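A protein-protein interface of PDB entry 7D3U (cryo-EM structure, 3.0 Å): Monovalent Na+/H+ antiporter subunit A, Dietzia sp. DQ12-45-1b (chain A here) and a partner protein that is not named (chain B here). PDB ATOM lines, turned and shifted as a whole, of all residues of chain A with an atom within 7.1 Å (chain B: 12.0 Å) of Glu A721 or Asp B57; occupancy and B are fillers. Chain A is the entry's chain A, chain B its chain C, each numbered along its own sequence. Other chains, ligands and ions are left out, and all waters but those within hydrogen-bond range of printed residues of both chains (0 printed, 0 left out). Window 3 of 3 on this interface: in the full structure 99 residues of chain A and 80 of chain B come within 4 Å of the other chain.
The backbone carbonyl oxygen of Pro B53 sits close to the backbone carbonyl oxygen of Ile A727, at 3.4 Å. OE1 of Glu A721 sits close to O of Ser B56 (3.3 Å).
O of Val A729 is in hydrogen-bond range of OG1 of Thr A732, at 2.9 Å. The backbone carbonyl oxygen (O) of Asn A728 lies close to the side-chain hydroxyl (OG1) of Thr A732, at 3.5 Å. The backbone carbonyl oxygen (O) of Gly A726 sits at hydrogen-bond distance from the backbone NH (N) of Glu A721 (3.5 Å).
CD2 of Leu A717 touches CB of Pro B53, 3.8 Å away. O of Leu A717 touches CD of Pro B58 (3.6 Å). CD1 of Leu A717 touches OG1 of Thr B63, 3.3 Å away. Asp B57 touches Glu A721 (OD1 to OE1, 3.6 Å). Ile A727 touches Leu B54 (CD1 to O, 3.6 Å). CB of Ile A727 touches O of Val B55 (3.7 Å). Asn A728 touches Leu B54. O of Pro B53 touches CG2 of Val A729, 3.3 Å away.
Phe A716 touches none of the printed residues of chain B. Of the printed residues of chain B, Glu A721 touches Ser B56 (3.3 Å) and Asp B57 (3.6 Å). No residue of chain B comes within 4 Å of Asp A723. No residue of chain B comes within 4 Å of Thr A724. No residue of chain B comes within 4 Å of Gly A725. Printed residues of chain B within 4 Å of Ile A727: Pro B53, Leu B54 and Val B55. Of the printed residues of chain B, Val A729 touches Pro B53. Of the printed residues of chain A, Ser B56 touches Glu A721. Of chain A, only Glu A721 comes within 4 Å of Asp B57. Ser B64 touches none of the printed residues of chain A. The nearest residue of chain B that does not touch Glu A721 is Val B55 (6.1 Å). The nearest residue of chain A that does not touch Asp B57 is Leu A717 (5.5 Å).
Of the 14 printed residues of chain B, 7 touch a printed residue of chain A. Printed residues of chain B that touch a printed residue of chain A: Pro B53, Leu B54, Val B55, Ser B56, Asp B57, Pro B58 and Thr B63. Of the 18 printed residues of chain A, 5 touch a printed residue of chain B. Hydrophobic or aromatic side chains of chain A that line the printed part of chain B: Leu A717, Ile A727 and Val A729. Among the printed residues, 10 pairs touch across the chains. Among the printed residues, no Asp or Glu carboxylate lies within 4 Å of a Lys or Arg side-chain nitrogen of the other chain.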
ATOM      1  N   PHE A 716     -36.122  25.073 -23.167  1.00  0.00           N
ATOM      2  CA  PHE A 716     -35.237  26.174 -23.535  1.00  0.00           C
ATOM      3  C   PHE A 716     -33.844  25.985 -22.949  1.00  0.00           C
ATOM      4  O   PHE A 716     -32.843  26.192 -23.643  1.00  0.00           O
ATOM      5  CB  PHE A 716     -35.830  27.506 -23.077  1.00  0.00           C
ATOM      6  CG  PHE A 716     -37.020  27.943 -23.875  1.00  0.00           C
ATOM      7  CD1 PHE A 716     -37.126  27.621 -25.213  1.00  0.00           C
ATOM      8  CD2 PHE A 716     -38.034  28.678 -23.289  1.00  0.00           C
ATOM      9  CE1 PHE A 716     -38.218  28.021 -25.950  1.00  0.00           C
ATOM     10  CE2 PHE A 716     -39.129  29.079 -24.023  1.00  0.00           C
ATOM     11  CZ  PHE A 716     -39.221  28.749 -25.355  1.00  0.00           C
ATOM     12  N   LEU A 717     -33.752  25.586 -21.678  1.00  0.00           N
ATOM     13  CA  LEU A 717     -32.430  25.370 -21.097  1.00  0.00           C
ATOM     14  C   LEU A 717     -31.755  24.126 -21.661  1.00  0.00           C
ATOM     15  O   LEU A 717     -30.521  24.043 -21.658  1.00  0.00           O
ATOM     16  CB  LEU A 717     -32.511  25.287 -19.570  1.00  0.00           C
ATOM     17  CG  LEU A 717     -33.345  26.341 -18.849  1.00  0.00           C
ATOM     18  CD1 LEU A 717     -33.429  26.023 -17.369  1.00  0.00           C
ATOM     19  CD2 LEU A 717     -32.764  27.723 -19.067  1.00  0.00           C
ATOM     20  N   ASP A 718     -32.527  23.156 -22.142  1.00  0.00           N
ATOM     21  CA  ASP A 718     -31.933  21.935 -22.672  1.00  0.00           C
ATOM     22  C   ASP A 718     -31.562  22.043 -24.145  1.00  0.00           C
ATOM     23  O   ASP A 718     -30.507  21.544 -24.552  1.00  0.00           O
ATOM     24  CB  ASP A 718     -32.889  20.757 -22.468  1.00  0.00           C
ATOM     25  CG  ASP A 718     -32.632  20.017 -21.176  1.00  0.00           C
ATOM     26  OD1 ASP A 718     -31.712  20.415 -20.433  1.00  0.00           O
ATOM     27  OD2 ASP A 718     -33.349  19.032 -20.903  1.00  0.00           O
ATOM     28  N   ASN A 719     -32.402  22.674 -24.957  1.00  0.00           N
ATOM     29  CA  ASN A 719     -32.225  22.711 -26.403  1.00  0.00           C
ATOM     30  C   ASN A 719     -32.026  24.133 -26.911  1.00  0.00           C
ATOM     31  O   ASN A 719     -32.615  24.540 -27.913  1.00  0.00           O
ATOM     32  CB  ASN A 719     -33.407  22.055 -27.110  1.00  0.00           C
ATOM     33  CG  ASN A 719     -33.569  20.598 -26.737  1.00  0.00           C
ATOM     34  OD1 ASN A 719     -34.556  20.209 -26.116  1.00  0.00           O
ATOM     35  ND2 ASN A 719     -32.596  19.781 -27.119  1.00  0.00           N
ATOM     36  N   ALA A 720     -31.193  24.915 -26.228  1.00  0.00           N
ATOM     37  CA  ALA A 720     -30.850  26.243 -26.722  1.00  0.00           C
ATOM     38  C   ALA A 720     -29.631  26.204 -27.635  1.00  0.00           C
ATOM     39  O   ALA A 720     -29.671  26.725 -28.752  1.00  0.00           O
ATOM     40  CB  ALA A 720     -30.601  27.200 -25.555  1.00  0.00           C
ATOM     41  N   GLU A 721     -28.541  25.588 -27.173  1.00  0.00           N
ATOM     42  CA  GLU A 721     -27.340  25.494 -27.992  1.00  0.00           C
ATOM     43  C   GLU A 721     -27.485  24.471 -29.110  1.00  0.00           C
ATOM     44  O   GLU A 721     -26.791  24.579 -30.126  1.00  0.00           O
ATOM     45  CB  GLU A 721     -26.133  25.146 -27.121  1.00  0.00           C
ATOM     46  CG  GLU A 721     -24.798  25.488 -27.757  1.00  0.00           C
ATOM     47  CD  GLU A 721     -23.620  25.111 -26.883  1.00  0.00           C
ATOM     48  OE1 GLU A 721     -23.836  24.438 -25.853  1.00  0.00           O
ATOM     49  OE2 GLU A 721     -22.479  25.485 -27.225  1.00  0.00           O
ATOM     50  N   GLN A 722     -28.368  23.485 -28.950  1.00  0.00           N
ATOM     51  CA  GLN A 722     -28.540  22.470 -29.980  1.00  0.00           C
ATOM     52  C   GLN A 722     -29.465  22.937 -31.096  1.00  0.00           C
ATOM     53  O   GLN A 722     -29.252  22.582 -32.260  1.00  0.00           O
ATOM     54  CB  GLN A 722     -29.071  21.179 -29.356  1.00  0.00           C
ATOM     55  CG  GLN A 722     -29.410  20.088 -30.357  1.00  0.00           C
ATOM     56  CD  GLN A 722     -28.218  19.675 -31.199  1.00  0.00           C
ATOM     57  OE1 GLN A 722     -28.337  19.475 -32.408  1.00  0.00           O
ATOM     58  NE2 GLN A 722     -27.060  19.541 -30.563  1.00  0.00           N
ATOM     59  N   ASP A 723     -30.482  23.735 -30.771  1.00  0.00           N
ATOM     60  CA  ASP A 723     -31.428  24.175 -31.790  1.00  0.00           C
ATOM     61  C   ASP A 723     -30.930  25.407 -32.535  1.00  0.00           C
ATOM     62  O   ASP A 723     -31.090  25.502 -33.755  1.00  0.00           O
ATOM     63  CB  ASP A 723     -32.789  24.460 -31.159  1.00  0.00           C
ATOM     64  CG  ASP A 723     -33.555  23.199 -30.835  1.00  0.00           C
ATOM     65  OD1 ASP A 723     -33.057  22.101 -31.155  1.00  0.00           O
ATOM     66  OD2 ASP A 723     -34.657  23.305 -30.257  1.00  0.00           O
ATOM     67  N   THR A 724     -30.328  26.360 -31.823  1.00  0.00           N
ATOM     68  CA  THR A 724     -29.966  27.641 -32.408  1.00  0.00           C
ATOM     69  C   THR A 724     -28.474  27.936 -32.407  1.00  0.00           C
ATOM     70  O   THR A 724     -28.059  28.909 -33.044  1.00  0.00           O
ATOM     71  CB  THR A 724     -30.688  28.782 -31.678  1.00  0.00           C
ATOM     72  OG1 THR A 724     -30.227  28.851 -30.325  1.00  0.00           O
ATOM     73  CG2 THR A 724     -32.186  28.547 -31.680  1.00  0.00           C
ATOM     74  N   GLY A 725     -27.658  27.142 -31.717  1.00  0.00           N
ATOM     75  CA  GLY A 725     -26.232  27.372 -31.673  1.00  0.00           C
ATOM     76  C   GLY A 725     -25.773  28.426 -30.689  1.00  0.00           C
ATOM     77  O   GLY A 725     -24.560  28.592 -30.509  1.00  0.00           O
ATOM     78  N   GLY A 726     -26.689  29.141 -30.049  1.00  0.00           N
ATOM     79  CA  GLY A 726     -26.346  30.168 -29.075  1.00  0.00           C
ATOM     80  C   GLY A 726     -26.683  29.703 -27.669  1.00  0.00           C
ATOM     81  O   GLY A 726     -27.642  28.954 -27.469  1.00  0.00           O
ATOM     82  N   ILE A 727     -25.886  30.152 -26.700  1.00  0.00           N
ATOM     83  CA  ILE A 727     -26.084  29.736 -25.318  1.00  0.00           C
ATOM     84  C   ILE A 727     -26.887  30.741 -24.501  1.00  0.00           C
ATOM     85  O   ILE A 727     -27.367  30.394 -23.414  1.00  0.00           O
ATOM     86  CB  ILE A 727     -24.735  29.473 -24.629  1.00  0.00           C
ATOM     87  CG1 ILE A 727     -23.937  30.768 -24.509  1.00  0.00           C
ATOM     88  CG2 ILE A 727     -23.944  28.432 -25.395  1.00  0.00           C
ATOM     89  CD1 ILE A 727     -22.602  30.595 -23.825  1.00  0.00           C
ATOM     90  N   ASN A 728     -27.047  31.968 -24.986  1.00  0.00           N
ATOM     91  CA  ASN A 728     -27.869  32.964 -24.302  1.00  0.00           C
ATOM     92  C   ASN A 728     -29.329  32.598 -24.517  1.00  0.00           C
ATOM     93  O   ASN A 728     -29.943  32.997 -25.507  1.00  0.00           O
ATOM     94  CB  ASN A 728     -27.560  34.360 -24.827  1.00  0.00           C
ATOM     95  CG  ASN A 728     -28.348  35.447 -24.116  1.00  0.00           C
ATOM     96  OD1 ASN A 728     -29.176  35.172 -23.251  1.00  0.00           O
ATOM     97  ND2 ASN A 728     -28.079  36.696 -24.474  1.00  0.00           N
ATOM     98  N   VAL A 729     -29.894  31.844 -23.572  1.00  0.00           N
ATOM     99  CA  VAL A 729     -31.243  31.315 -23.739  1.00  0.00           C
ATOM    100  C   VAL A 729     -32.253  32.440 -23.910  1.00  0.00           C
ATOM    101  O   VAL A 729     -33.190  32.331 -24.708  1.00  0.00           O
ATOM    102  CB  VAL A 729     -31.605  30.406 -22.554  1.00  0.00           C
ATOM    103  CG1 VAL A 729     -32.954  29.762 -22.781  1.00  0.00           C
ATOM    104  CG2 VAL A 729     -30.536  29.351 -22.363  1.00  0.00           C
ATOM    105  N   THR A 732     -31.934  33.839 -27.501  1.00  0.00           N
ATOM    106  CA  THR A 732     -32.442  32.892 -28.489  1.00  0.00           C
ATOM    107  C   THR A 732     -33.960  32.802 -28.436  1.00  0.00           C
ATOM    108  O   THR A 732     -34.619  32.727 -29.479  1.00  0.00           O
ATOM    109  CB  THR A 732     -31.819  31.513 -28.288  1.00  0.00           C
ATOM    110  OG1 THR A 732     -32.295  30.946 -27.061  1.00  0.00           O
ATOM    111  CG2 THR A 732     -30.306  31.600 -28.268  1.00  0.00           C
ATOM    112  N   TYR A 737     -36.914  31.479 -31.096  1.00  0.00           N
ATOM    113  CA  TYR A 737     -38.151  30.759 -30.795  1.00  0.00           C
ATOM    114  C   TYR A 737     -39.361  31.682 -30.890  1.00  0.00           C
ATOM    115  O   TYR A 737     -40.217  31.517 -31.764  1.00  0.00           O
ATOM    116  CB  TYR A 737     -38.068  30.127 -29.401  1.00  0.00           C
ATOM    117  CG  TYR A 737     -36.998  29.073 -29.246  1.00  0.00           C
ATOM    118  CD1 TYR A 737     -37.082  27.866 -29.921  1.00  0.00           C
ATOM    119  CD2 TYR A 737     -35.915  29.282 -28.409  1.00  0.00           C
ATOM    120  CE1 TYR A 737     -36.111  26.902 -29.772  1.00  0.00           C
ATOM    121  CE2 TYR A 737     -34.941  28.323 -28.255  1.00  0.00           C
ATOM    122  CZ  TYR A 737     -35.044  27.138 -28.939  1.00  0.00           C
ATOM    123  OH  TYR A 737     -34.071  26.182 -28.784  1.00  0.00           O
ATOM    124  N   ASN A 815     -24.385  34.787 -27.352  1.00  0.00           N
ATOM    125  CA  ASN A 815     -23.682  34.004 -26.343  1.00  0.00           C
ATOM    126  C   ASN A 815     -23.299  34.851 -25.135  1.00  0.00           C
ATOM    127  O   ASN A 815     -22.418  34.460 -24.364  1.00  0.00           O
ATOM    128  CB  ASN A 815     -22.436  33.345 -26.938  1.00  0.00           C
ATOM    129  CG  ASN A 815     -22.742  32.536 -28.181  1.00  0.00           C
ATOM    130  OD1 ASN A 815     -23.128  33.085 -29.212  1.00  0.00           O
ATOM    131  ND2 ASN A 815     -22.569  31.224 -28.091  1.00  0.00           N
ATOM    132  N   TYR A 881     -22.882  28.573 -42.011  1.00  0.00           N
ATOM    133  CA  TYR A 881     -21.568  28.468 -41.394  1.00  0.00           C
ATOM    134  C   TYR A 881     -20.494  28.947 -42.360  1.00  0.00           C
ATOM    135  O   TYR A 881     -20.430  28.491 -43.506  1.00  0.00           O
ATOM    136  CB  TYR A 881     -21.292  27.027 -40.962  1.00  0.00           C
ATOM    137  CG  TYR A 881     -22.214  26.532 -39.871  1.00  0.00           C
ATOM    138  CD1 TYR A 881     -23.520  26.153 -40.155  1.00  0.00           C
ATOM    139  CD2 TYR A 881     -21.783  26.452 -38.555  1.00  0.00           C
ATOM    140  CE1 TYR A 881     -24.367  25.704 -39.163  1.00  0.00           C
ATOM    141  CE2 TYR A 881     -22.624  26.003 -37.554  1.00  0.00           C
ATOM    142  CZ  TYR A 881     -23.915  25.631 -37.864  1.00  0.00           C
ATOM    143  OH  TYR A 881     -24.757  25.184 -36.871  1.00  0.00           O
ATOM    144  N   GLU B  51     -29.538  31.411 -10.673  1.00  0.00           N
ATOM    145  CA  GLU B  51     -28.407  31.335 -11.584  1.00  0.00           C
ATOM    146  C   GLU B  51     -28.838  31.761 -12.980  1.00  0.00           C
ATOM    147  O   GLU B  51     -29.930  31.416 -13.437  1.00  0.00           O
ATOM    148  CB  GLU B  51     -27.824  29.923 -11.620  1.00  0.00           C
ATOM    149  CG  GLU B  51     -26.368  29.873 -12.045  1.00  0.00           C
ATOM    150  CD  GLU B  51     -25.724  28.532 -11.766  1.00  0.00           C
ATOM    151  OE1 GLU B  51     -26.451  27.589 -11.389  1.00  0.00           O
ATOM    152  OE2 GLU B  51     -24.491  28.419 -11.923  1.00  0.00           O
ATOM    153  N   ALA B  52     -27.978  32.518 -13.650  1.00  0.00           N
ATOM    154  CA  ALA B  52     -28.316  33.028 -14.967  1.00  0.00           C
ATOM    155  C   ALA B  52     -28.250  31.905 -15.999  1.00  0.00           C
ATOM    156  O   ALA B  52     -27.366  31.047 -15.927  1.00  0.00           O
ATOM    157  CB  ALA B  52     -27.370  34.158 -15.362  1.00  0.00           C
ATOM    158  N   PRO B  53     -29.173  31.881 -16.971  1.00  0.00           N
ATOM    159  CA  PRO B  53     -29.154  30.862 -18.025  1.00  0.00           C
ATOM    160  C   PRO B  53     -28.235  31.225 -19.188  1.00  0.00           C
ATOM    161  O   PRO B  53     -28.627  31.178 -20.357  1.00  0.00           O
ATOM    162  CB  PRO B  53     -30.625  30.809 -18.464  1.00  0.00           C
ATOM    163  CG  PRO B  53     -31.092  32.203 -18.273  1.00  0.00           C
ATOM    164  CD  PRO B  53     -30.368  32.738 -17.059  1.00  0.00           C
ATOM    165  N   LEU B  54     -26.995  31.593 -18.871  1.00  0.00           N
ATOM    166  CA  LEU B  54     -26.023  32.004 -19.876  1.00  0.00           C
ATOM    167  C   LEU B  54     -24.804  31.094 -19.919  1.00  0.00           C
ATOM    168  O   LEU B  54     -23.812  31.438 -20.571  1.00  0.00           O
ATOM    169  CB  LEU B  54     -25.586  33.449 -19.626  1.00  0.00           C
ATOM    170  CG  LEU B  54     -26.692  34.501 -19.608  1.00  0.00           C
ATOM    171  CD1 LEU B  54     -26.303  35.670 -18.728  1.00  0.00           C
ATOM    172  CD2 LEU B  54     -26.969  34.976 -21.011  1.00  0.00           C
ATOM    173  N   VAL B  55     -24.848  29.947 -19.247  1.00  0.00           N
ATOM    174  CA  VAL B  55     -23.727  29.015 -19.238  1.00  0.00           C
ATOM    175  C   VAL B  55     -23.825  28.137 -20.478  1.00  0.00           C
ATOM    176  O   VAL B  55     -24.867  28.103 -21.142  1.00  0.00           O
ATOM    177  CB  VAL B  55     -23.714  28.174 -17.950  1.00  0.00           C
ATOM    178  CG1 VAL B  55     -22.614  27.121 -18.004  1.00  0.00           C
ATOM    179  CG2 VAL B  55     -23.544  29.070 -16.735  1.00  0.00           C
ATOM    180  N   SER B  56     -22.740  27.430 -20.805  1.00  0.00           N
ATOM    181  CA  SER B  56     -22.721  26.594 -22.000  1.00  0.00           C
ATOM    182  C   SER B  56     -23.802  25.521 -21.938  1.00  0.00           C
ATOM    183  O   SER B  56     -24.672  25.443 -22.812  1.00  0.00           O
ATOM    184  CB  SER B  56     -21.339  25.965 -22.174  1.00  0.00           C
ATOM    185  OG  SER B  56     -20.758  25.661 -20.919  1.00  0.00           O
ATOM    186  N   ASP B  57     -23.763  24.681 -20.904  1.00  0.00           N
ATOM    187  CA  ASP B  57     -24.790  23.671 -20.662  1.00  0.00           C
ATOM    188  C   ASP B  57     -25.522  24.032 -19.377  1.00  0.00           C
ATOM    189  O   ASP B  57     -25.091  23.645 -18.282  1.00  0.00           O
ATOM    190  CB  ASP B  57     -24.182  22.270 -20.565  1.00  0.00           C
ATOM    191  CG  ASP B  57     -23.651  21.771 -21.894  1.00  0.00           C
ATOM    192  OD1 ASP B  57     -23.430  22.604 -22.798  1.00  0.00           O
ATOM    193  OD2 ASP B  57     -23.458  20.546 -22.035  1.00  0.00           O
ATOM    194  N   PRO B  58     -26.623  24.780 -19.454  1.00  0.00           N
ATOM    195  CA  PRO B  58     -27.305  25.212 -18.229  1.00  0.00           C
ATOM    196  C   PRO B  58     -27.791  24.023 -17.418  1.00  0.00           C
ATOM    197  O   PRO B  58     -28.227  23.009 -17.966  1.00  0.00           O
ATOM    198  CB  PRO B  58     -28.476  26.055 -18.753  1.00  0.00           C
ATOM    199  CG  PRO B  58     -28.092  26.430 -20.148  1.00  0.00           C
ATOM    200  CD  PRO B  58     -27.295  25.277 -20.665  1.00  0.00           C
ATOM    201  N   ASP B  59     -27.698  24.154 -16.100  1.00  0.00           N
ATOM    202  CA  ASP B  59     -28.081  23.090 -15.184  1.00  0.00           C
ATOM    203  C   ASP B  59     -29.501  23.325 -14.688  1.00  0.00           C
ATOM    204  O   ASP B  59     -29.717  24.173 -13.814  1.00  0.00           O
ATOM    205  CB  ASP B  59     -27.105  23.020 -14.010  1.00  0.00           C
ATOM    206  CG  ASP B  59     -27.234  21.736 -13.218  1.00  0.00           C
ATOM    207  OD1 ASP B  59     -28.293  21.523 -12.591  1.00  0.00           O
ATOM    208  OD2 ASP B  59     -26.275  20.938 -13.223  1.00  0.00           O
ATOM    209  N   PRO B  60     -30.488  22.600 -15.213  1.00  0.00           N
ATOM    210  CA  PRO B  60     -31.870  22.808 -14.769  1.00  0.00           C
ATOM    211  C   PRO B  60     -32.019  22.551 -13.278  1.00  0.00           C
ATOM    212  O   PRO B  60     -31.161  21.946 -12.633  1.00  0.00           O
ATOM    213  CB  PRO B  60     -32.666  21.793 -15.596  1.00  0.00           C
ATOM    214  CG  PRO B  60     -31.672  20.758 -15.981  1.00  0.00           C
ATOM    215  CD  PRO B  60     -30.376  21.486 -16.166  1.00  0.00           C
ATOM    216  N   ALA B  61     -33.131  23.038 -12.733  1.00  0.00           N
ATOM    217  CA  ALA B  61     -33.409  23.066 -11.300  1.00  0.00           C
ATOM    218  C   ALA B  61     -32.387  23.888 -10.524  1.00  0.00           C
ATOM    219  O   ALA B  61     -32.391  23.866  -9.288  1.00  0.00           O
ATOM    220  CB  ALA B  61     -33.502  21.651 -10.710  1.00  0.00           C
ATOM    221  N   LEU B  62     -31.508  24.608 -11.218  1.00  0.00           N
ATOM    222  CA  LEU B  62     -30.566  25.519 -10.584  1.00  0.00           C
ATOM    223  C   LEU B  62     -30.485  26.885 -11.247  1.00  0.00           C
ATOM    224  O   LEU B  62     -30.087  27.845 -10.576  1.00  0.00           O
ATOM    225  CB  LEU B  62     -29.159  24.902 -10.556  1.00  0.00           C
ATOM    226  CG  LEU B  62     -28.183  25.469  -9.525  1.00  0.00           C
ATOM    227  CD1 LEU B  62     -28.774  25.381  -8.130  1.00  0.00           C
ATOM    228  CD2 LEU B  62     -26.850  24.744  -9.594  1.00  0.00           C
ATOM    229  N   THR B  63     -30.853  27.013 -12.519  1.00  0.00           N
ATOM    230  CA  THR B  63     -30.799  28.282 -13.229  1.00  0.00           C
ATOM    231  C   THR B  63     -32.193  28.877 -13.379  1.00  0.00           C
ATOM    232  O   THR B  63     -33.193  28.159 -13.443  1.00  0.00           O
ATOM    233  CB  THR B  63     -30.170  28.119 -14.612  1.00  0.00           C
ATOM    234  OG1 THR B  63     -31.156  27.633 -15.530  1.00  0.00           O
ATOM    235  CG2 THR B  63     -29.004  27.154 -14.560  1.00  0.00           C
ATOM    236  N   SER B  64     -32.243  30.205 -13.439  1.00  0.00           N
ATOM    237  CA  SER B  64     -33.509  30.902 -13.599  1.00  0.00           C
ATOM    238  C   SER B  64     -34.122  30.584 -14.956  1.00  0.00           C
ATOM    239  O   SER B  64     -33.419  30.388 -15.951  1.00  0.00           O
ATOM    240  CB  SER B  64     -33.311  32.409 -13.455  1.00  0.00           C
ATOM    241  OG  SER B  64     -34.427  33.122 -13.957  1.00  0.00           O
